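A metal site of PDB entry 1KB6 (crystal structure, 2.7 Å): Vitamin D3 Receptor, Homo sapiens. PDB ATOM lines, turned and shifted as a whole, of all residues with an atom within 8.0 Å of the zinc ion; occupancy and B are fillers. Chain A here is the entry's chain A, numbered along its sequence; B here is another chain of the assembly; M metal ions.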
ATOM      1  N   ILE A   8      23.206  -5.603  20.534  1.00  0.00           N
ATOM      2  CA  ILE A   8      22.962  -5.154  19.171  1.00  0.00           C
ATOM      3  C   ILE A   8      23.268  -6.325  18.227  1.00  0.00           C
ATOM      4  O   ILE A   8      24.280  -6.989  18.337  1.00  0.00           O
ATOM      5  CB  ILE A   8      23.774  -3.874  18.806  1.00  0.00           C
ATOM      6  CG1 ILE A   8      24.681  -4.140  17.603  1.00  0.00           C
ATOM      7  CG2 ILE A   8      24.533  -3.381  20.016  1.00  0.00           C
ATOM      8  CD1 ILE A   8      26.226  -4.081  17.913  1.00  0.00           C
ATOM      9  N   CYS A   9      22.343  -6.599  17.328  1.00  0.00           N
ATOM     10  CA  CYS A   9      22.517  -7.704  16.404  1.00  0.00           C
ATOM     11  C   CYS A   9      23.809  -7.594  15.610  1.00  0.00           C
ATOM     12  O   CYS A   9      24.067  -6.587  14.966  1.00  0.00           O
ATOM     13  CB  CYS A   9      21.324  -7.787  15.433  1.00  0.00           C
ATOM     14  SG  CYS A   9      21.517  -8.975  14.081  1.00  0.00           S
ATOM     15  N   GLY A  10      24.587  -8.675  15.648  1.00  0.00           N
ATOM     16  CA  GLY A  10      25.850  -8.762  14.948  1.00  0.00           C
ATOM     17  C   GLY A  10      25.735  -8.935  13.462  1.00  0.00           C
ATOM     18  O   GLY A  10      26.702  -8.973  12.726  1.00  0.00           O
ATOM     19  N   VAL A  11      24.521  -9.005  12.984  1.00  0.00           N
ATOM     20  CA  VAL A  11      24.351  -9.215  11.574  1.00  0.00           C
ATOM     21  C   VAL A  11      23.907  -7.959  10.914  1.00  0.00           C
ATOM     22  O   VAL A  11      24.563  -7.496  10.004  1.00  0.00           O
ATOM     23  CB  VAL A  11      23.322 -10.393  11.299  1.00  0.00           C
ATOM     24  CG1 VAL A  11      23.023 -10.505   9.806  1.00  0.00           C
ATOM     25  CG2 VAL A  11      23.897 -11.717  11.847  1.00  0.00           C
ATOM     26  N   CYS A  12      22.806  -7.393  11.395  1.00  0.00           N
ATOM     27  CA  CYS A  12      22.270  -6.180  10.811  1.00  0.00           C
ATOM     28  C   CYS A  12      22.333  -4.938  11.695  1.00  0.00           C
ATOM     29  O   CYS A  12      22.065  -3.827  11.240  1.00  0.00           O
ATOM     30  CB  CYS A  12      20.827  -6.413  10.427  1.00  0.00           C
ATOM     31  SG  CYS A  12      19.837  -6.558  11.844  1.00  0.00           S
ATOM     32  N   GLY A  13      22.643  -5.105  12.960  1.00  0.00           N
ATOM     33  CA  GLY A  13      22.711  -3.917  13.776  1.00  0.00           C
ATOM     34  C   GLY A  13      21.426  -3.502  14.452  1.00  0.00           C
ATOM     35  O   GLY A  13      21.448  -2.595  15.268  1.00  0.00           O
ATOM     36  N   ASP A  14      20.314  -4.128  14.117  1.00  0.00           N
ATOM     37  CA  ASP A  14      19.027  -3.850  14.764  1.00  0.00           C
ATOM     38  C   ASP A  14      19.167  -4.173  16.274  1.00  0.00           C
ATOM     39  O   ASP A  14      20.221  -4.605  16.767  1.00  0.00           O
ATOM     40  CB  ASP A  14      17.944  -4.737  14.132  1.00  0.00           C
ATOM     41  CG  ASP A  14      16.550  -4.244  14.414  1.00  0.00           C
ATOM     42  OD1 ASP A  14      16.362  -3.435  15.341  1.00  0.00           O
ATOM     43  OD2 ASP A  14      15.610  -4.675  13.699  1.00  0.00           O
ATOM     44  N   ARG A  15      18.101  -3.982  17.018  1.00  0.00           N
ATOM     45  CA  ARG A  15      18.162  -4.229  18.441  1.00  0.00           C
ATOM     46  C   ARG A  15      18.134  -5.738  18.718  1.00  0.00           C
ATOM     47  O   ARG A  15      17.178  -6.452  18.310  1.00  0.00           O
ATOM     48  CB  ARG A  15      16.999  -3.497  19.103  1.00  0.00           C
ATOM     49  CG  ARG A  15      17.199  -3.231  20.557  1.00  0.00           C
ATOM     50  CD  ARG A  15      16.580  -4.348  21.368  1.00  0.00           C
ATOM     51  NE  ARG A  15      15.128  -4.452  21.176  1.00  0.00           N
ATOM     52  CZ  ARG A  15      14.351  -5.328  21.823  1.00  0.00           C
ATOM     53  NH1 ARG A  15      14.871  -6.175  22.705  1.00  0.00           N
ATOM     54  NH2 ARG A  15      13.042  -5.351  21.583  1.00  0.00           N
ATOM     55  N   ALA A  16      19.162  -6.241  19.387  1.00  0.00           N
ATOM     56  CA  ALA A  16      19.228  -7.682  19.666  1.00  0.00           C
ATOM     57  C   ALA A  16      18.384  -8.254  20.847  1.00  0.00           C
ATOM     58  O   ALA A  16      18.419  -7.728  21.954  1.00  0.00           O
ATOM     59  CB  ALA A  16      20.709  -8.108  19.823  1.00  0.00           C
ATOM     60  N   MET A  24      24.605 -13.121  19.285  1.00  0.00           N
ATOM     61  CA  MET A  24      23.738 -12.015  19.622  1.00  0.00           C
ATOM     62  C   MET A  24      23.048 -11.567  18.353  1.00  0.00           C
ATOM     63  O   MET A  24      23.641 -10.926  17.526  1.00  0.00           O
ATOM     64  CB  MET A  24      24.572 -10.872  20.200  1.00  0.00           C
ATOM     65  CG  MET A  24      23.782  -9.740  20.827  1.00  0.00           C
ATOM     66  SD  MET A  24      22.583 -10.331  22.105  1.00  0.00           S
ATOM     67  CE  MET A  24      23.635 -11.391  23.130  1.00  0.00           C
ATOM     68  N   THR A  25      21.769 -11.890  18.202  1.00  0.00           N
ATOM     69  CA  THR A  25      21.049 -11.466  17.004  1.00  0.00           C
ATOM     70  C   THR A  25      19.633 -10.913  17.317  1.00  0.00           C
ATOM     71  O   THR A  25      19.131 -11.013  18.447  1.00  0.00           O
ATOM     72  CB  THR A  25      20.931 -12.644  16.040  1.00  0.00           C
ATOM     73  OG1 THR A  25      20.198 -13.674  16.690  1.00  0.00           O
ATOM     74  CG2 THR A  25      22.288 -13.174  15.644  1.00  0.00           C
ATOM     75  N   CYS A  26      19.025 -10.340  16.283  1.00  0.00           N
ATOM     76  CA  CYS A  26      17.700  -9.744  16.360  1.00  0.00           C
ATOM     77  C   CYS A  26      16.733 -10.834  16.015  1.00  0.00           C
ATOM     78  O   CYS A  26      17.172 -11.900  15.551  1.00  0.00           O
ATOM     79  CB  CYS A  26      17.563  -8.563  15.367  1.00  0.00           C
ATOM     80  SG  CYS A  26      17.540  -8.864  13.509  1.00  0.00           S
ATOM     81  N   GLU A  27      15.445 -10.598  16.234  1.00  0.00           N
ATOM     82  CA  GLU A  27      14.485 -11.609  15.872  1.00  0.00           C
ATOM     83  C   GLU A  27      14.530 -11.872  14.368  1.00  0.00           C
ATOM     84  O   GLU A  27      14.429 -12.984  13.938  1.00  0.00           O
ATOM     85  CB  GLU A  27      13.070 -11.207  16.308  1.00  0.00           C
ATOM     86  CG  GLU A  27      12.868 -11.362  17.801  1.00  0.00           C
ATOM     87  CD  GLU A  27      13.102 -12.805  18.311  1.00  0.00           C
ATOM     88  OE1 GLU A  27      12.411 -13.725  17.799  1.00  0.00           O
ATOM     89  OE2 GLU A  27      13.966 -13.008  19.219  1.00  0.00           O
ATOM     90  N   GLY A  28      14.705 -10.840  13.572  1.00  0.00           N
ATOM     91  CA  GLY A  28      14.740 -11.083  12.149  1.00  0.00           C
ATOM     92  C   GLY A  28      15.911 -11.942  11.697  1.00  0.00           C
ATOM     93  O   GLY A  28      15.816 -12.760  10.774  1.00  0.00           O
ATOM     94  N   CYS A  29      17.058 -11.794  12.312  1.00  0.00           N
ATOM     95  CA  CYS A  29      18.122 -12.586  11.768  1.00  0.00           C
ATOM     96  C   CYS A  29      18.072 -14.037  12.283  1.00  0.00           C
ATOM     97  O   CYS A  29      18.599 -14.934  11.633  1.00  0.00           O
ATOM     98  CB  CYS A  29      19.454 -11.872  12.018  1.00  0.00           C
ATOM     99  SG  CYS A  29      19.591 -10.240  11.105  1.00  0.00           S
ATOM    100  N   LYS A  30      17.438 -14.290  13.415  1.00  0.00           N
ATOM    101  CA  LYS A  30      17.352 -15.657  13.874  1.00  0.00           C
ATOM    102  C   LYS A  30      16.425 -16.331  12.864  1.00  0.00           C
ATOM    103  O   LYS A  30      16.747 -17.360  12.267  1.00  0.00           O
ATOM    104  CB  LYS A  30      16.795 -15.685  15.303  1.00  0.00           C
ATOM    105  CG  LYS A  30      15.549 -16.479  15.607  1.00  0.00           C
ATOM    106  CD  LYS A  30      15.043 -16.061  16.985  1.00  0.00           C
ATOM    107  CE  LYS A  30      13.815 -16.870  17.424  1.00  0.00           C
ATOM    108  NZ  LYS A  30      13.108 -16.318  18.648  1.00  0.00           N
ATOM    109  N   PHE A  32      15.519 -15.365   9.813  1.00  0.00           N
ATOM    110  CA  PHE A  32      16.119 -15.485   8.514  1.00  0.00           C
ATOM    111  C   PHE A  32      17.103 -16.649   8.462  1.00  0.00           C
ATOM    112  O   PHE A  32      17.073 -17.465   7.549  1.00  0.00           O
ATOM    113  CB  PHE A  32      16.894 -14.231   8.187  1.00  0.00           C
ATOM    114  CG  PHE A  32      17.696 -14.370   6.973  1.00  0.00           C
ATOM    115  CD1 PHE A  32      17.125 -14.207   5.752  1.00  0.00           C
ATOM    116  CD2 PHE A  32      19.023 -14.677   7.053  1.00  0.00           C
ATOM    117  CE1 PHE A  32      17.874 -14.357   4.645  1.00  0.00           C
ATOM    118  CE2 PHE A  32      19.772 -14.827   5.947  1.00  0.00           C
ATOM    119  CZ  PHE A  32      19.217 -14.662   4.732  1.00  0.00           C
ATOM    120  N   ILE A  53      25.227  -4.866   5.881  1.00  0.00           N
ATOM    121  CA  ILE A  53      23.860  -5.127   6.291  1.00  0.00           C
ATOM    122  C   ILE A  53      23.422  -4.167   7.341  1.00  0.00           C
ATOM    123  O   ILE A  53      24.163  -3.844   8.241  1.00  0.00           O
ATOM    124  CB  ILE A  53      23.721  -6.605   6.853  1.00  0.00           C
ATOM    125  CG1 ILE A  53      24.632  -7.550   6.047  1.00  0.00           C
ATOM    126  CG2 ILE A  53      22.298  -7.129   6.691  1.00  0.00           C
ATOM    127  CD1 ILE A  53      24.352  -7.510   4.583  1.00  0.00           C
ATOM    128  N   THR A  54      22.186  -3.688   7.213  1.00  0.00           N
ATOM    129  CA  THR A  54      21.618  -2.754   8.189  1.00  0.00           C
ATOM    130  C   THR A  54      20.164  -3.110   8.447  1.00  0.00           C
ATOM    131  O   THR A  54      19.515  -3.834   7.664  1.00  0.00           O
ATOM    132  CB  THR A  54      21.676  -1.263   7.733  1.00  0.00           C
ATOM    133  OG1 THR A  54      20.884  -1.057   6.557  1.00  0.00           O
ATOM    134  CG2 THR A  54      23.073  -0.858   7.470  1.00  0.00           C
ATOM    135  N   LYS A  55      19.635  -2.598   9.541  1.00  0.00           N
ATOM    136  CA  LYS A  55      18.254  -2.846   9.870  1.00  0.00           C
ATOM    137  C   LYS A  55      17.336  -2.475   8.706  1.00  0.00           C
ATOM    138  O   LYS A  55      16.226  -2.988   8.620  1.00  0.00           O
ATOM    139  CB  LYS A  55      17.874  -2.080  11.131  1.00  0.00           C
ATOM    140  CG  LYS A  55      16.520  -2.480  11.744  1.00  0.00           C
ATOM    141  CD  LYS A  55      15.278  -1.939  10.979  1.00  0.00           C
ATOM    142  CE  LYS A  55      14.002  -2.111  11.822  1.00  0.00           C
ATOM    143  NZ  LYS A  55      14.316  -1.943  13.286  1.00  0.00           N
ATOM    144  N   ARG A  58      18.706  -5.313   5.185  1.00  0.00           N
ATOM    145  CA  ARG A  58      18.810  -6.754   5.334  1.00  0.00           C
ATOM    146  C   ARG A  58      17.864  -7.527   4.465  1.00  0.00           C
ATOM    147  O   ARG A  58      18.243  -8.494   3.869  1.00  0.00           O
ATOM    148  CB  ARG A  58      18.590  -7.136   6.779  1.00  0.00           C
ATOM    149  CG  ARG A  58      17.302  -6.650   7.337  1.00  0.00           C
ATOM    150  CD  ARG A  58      17.248  -6.935   8.812  1.00  0.00           C
ATOM    151  NE  ARG A  58      15.894  -6.741   9.316  1.00  0.00           N
ATOM    152  CZ  ARG A  58      15.615  -6.549  10.597  1.00  0.00           C
ATOM    153  NH1 ARG A  58      16.613  -6.528  11.483  1.00  0.00           N
ATOM    154  NH2 ARG A  58      14.343  -6.365  10.973  1.00  0.00           N
ATOM    155  N   ARG A  65      23.529 -11.256   3.839  1.00  0.00           N
ATOM    156  CA  ARG A  65      22.991 -11.395   5.173  1.00  0.00           C
ATOM    157  C   ARG A  65      23.304 -12.800   5.655  1.00  0.00           C
ATOM    158  O   ARG A  65      23.766 -12.987   6.750  1.00  0.00           O
ATOM    159  CB  ARG A  65      21.491 -11.181   5.158  1.00  0.00           C
ATOM    160  CG  ARG A  65      20.809 -11.314   6.505  1.00  0.00           C
ATOM    161  CD  ARG A  65      19.367 -10.889   6.378  1.00  0.00           C
ATOM    162  NE  ARG A  65      18.791 -10.695   7.697  1.00  0.00           N
ATOM    163  CZ  ARG A  65      17.481 -10.552   7.980  1.00  0.00           C
ATOM    164  NH1 ARG A  65      16.531 -10.583   7.037  1.00  0.00           N
ATOM    165  NH2 ARG A  65      17.109 -10.437   9.245  1.00  0.00           N
ATOM    166  N   CYS A  69      25.730 -14.178   8.772  1.00  0.00           N
ATOM    167  CA  CYS A  69      25.366 -14.948   9.985  1.00  0.00           C
ATOM    168  C   CYS A  69      26.411 -16.014  10.233  1.00  0.00           C
ATOM    169  O   CYS A  69      26.826 -16.295  11.343  1.00  0.00           O
ATOM    170  CB  CYS A  69      24.021 -15.650   9.860  1.00  0.00           C
ATOM    171  SG  CYS A  69      22.583 -14.619   9.557  1.00  0.00           S
ATOM    172  N   ILE A  72      29.659 -14.398  11.800  1.00  0.00           N
ATOM    173  CA  ILE A  72      29.711 -14.005  13.225  1.00  0.00           C
ATOM    174  C   ILE A  72      29.551 -15.223  14.125  1.00  0.00           C
ATOM    175  O   ILE A  72      29.455 -15.125  15.367  1.00  0.00           O
ATOM    176  CB  ILE A  72      28.636 -12.969  13.594  1.00  0.00           C
ATOM    177  CG1 ILE A  72      27.257 -13.583  13.596  1.00  0.00           C
ATOM    178  CG2 ILE A  72      28.643 -11.873  12.591  1.00  0.00           C
ATOM    179  CD1 ILE A  72      26.216 -12.719  14.273  1.00  0.00           C
ATOM    180  N   MET A  74      27.015 -17.909  13.815  1.00  0.00           N
ATOM    181  CA  MET A  74      25.779 -18.623  14.088  1.00  0.00           C
ATOM    182  C   MET A  74      26.063 -20.037  13.595  1.00  0.00           C
ATOM    183  O   MET A  74      26.839 -20.250  12.671  1.00  0.00           O
ATOM    184  CB  MET A  74      24.595 -17.984  13.373  1.00  0.00           C
ATOM    185  CG  MET A  74      24.376 -16.613  13.881  1.00  0.00           C
ATOM    186  SD  MET A  74      23.199 -15.800  12.911  1.00  0.00           S
ATOM    187  CE  MET A  74      21.675 -16.159  13.893  1.00  0.00           C
ATOM    188  P    DC B  11      13.146  -9.179   8.397  1.00  0.00           P
ATOM    189  OP1  DC B  11      13.513  -7.746   8.346  1.00  0.00           O
ATOM    190  OP2  DC B  11      14.177 -10.197   8.658  1.00  0.00           O
ATOM    191  O5'  DC B  11      12.050  -9.280   9.518  1.00  0.00           O
ATOM    192  C5'  DC B  11      11.146  -8.233   9.687  1.00  0.00           C
ATOM    193  C4'  DC B  11      10.270  -8.524  10.876  1.00  0.00           C
ATOM    194  O4'  DC B  11       9.639  -9.798  10.636  1.00  0.00           O
ATOM    195  C3'  DC B  11      10.971  -8.651  12.233  1.00  0.00           C
ATOM    196  O3'  DC B  11      10.143  -7.996  13.179  1.00  0.00           O
ATOM    197  C2'  DC B  11      10.970 -10.165  12.475  1.00  0.00           C
ATOM    198  C1'  DC B  11       9.665 -10.538  11.834  1.00  0.00           C
ATOM    199  N1   DC B  11       9.395 -11.900  11.464  1.00  0.00           N
ATOM    200  C2   DC B  11       8.077 -12.334  11.490  1.00  0.00           C
ATOM    201  O2   DC B  11       7.238 -11.596  12.027  1.00  0.00           O
ATOM    202  N3   DC B  11       7.758 -13.541  10.971  1.00  0.00           N
ATOM    203  C4   DC B  11       8.714 -14.332  10.493  1.00  0.00           C
ATOM    204  N4   DC B  11       8.368 -15.491   9.958  1.00  0.00           N
ATOM    205  C5   DC B  11      10.077 -13.944  10.534  1.00  0.00           C
ATOM    206  C6   DC B  11      10.373 -12.733  11.029  1.00  0.00           C
HETATM  207 ZN    ZN M   1      19.779  -8.616  12.753  1.00  0.00          ZN
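Residues that only touch the zinc ion: Arg 58 (3.9995 Å).
The zinc ion is bound by the side-chain sulfur (SG) of Cys 9 (2.2 Å), the side-chain sulfur (SG) of Cys 12 (2.3 Å), the side-chain sulfur (SG) of Cys 29 (2.3 Å) and the side-chain sulfur (SG) of Cys 26 (2.4 Å).
The zinc ion has four donor atoms within binding distance.
SG of Cys 9 sits close to N of Val 11 of chain A (3.2 Å).
N of Cys 9 sits at hydrogen-bond distance from O of Asp 14 (3.0 Å).
O of Cys 12 is in hydrogen-bond range of N of Lys 55.
The guanidinium group (NH2) of Arg 65 lies close to the side-chain sulfur (SG) of Cys 29, 3.1 Å away.
SG of Cys 26 lies close to NH1 of Arg 58 (3.2 Å).
The backbone NH of Gly 28 sits close to the side-chain sulfur of Cys 26.
NH1 of Arg 58 lies within salt-bridge range of OD2 of Asp 14, 3.1 Å away.
OP1 of DC 11 of chain B lies within salt-bridge range of NE of Arg 58 (2.8 Å).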
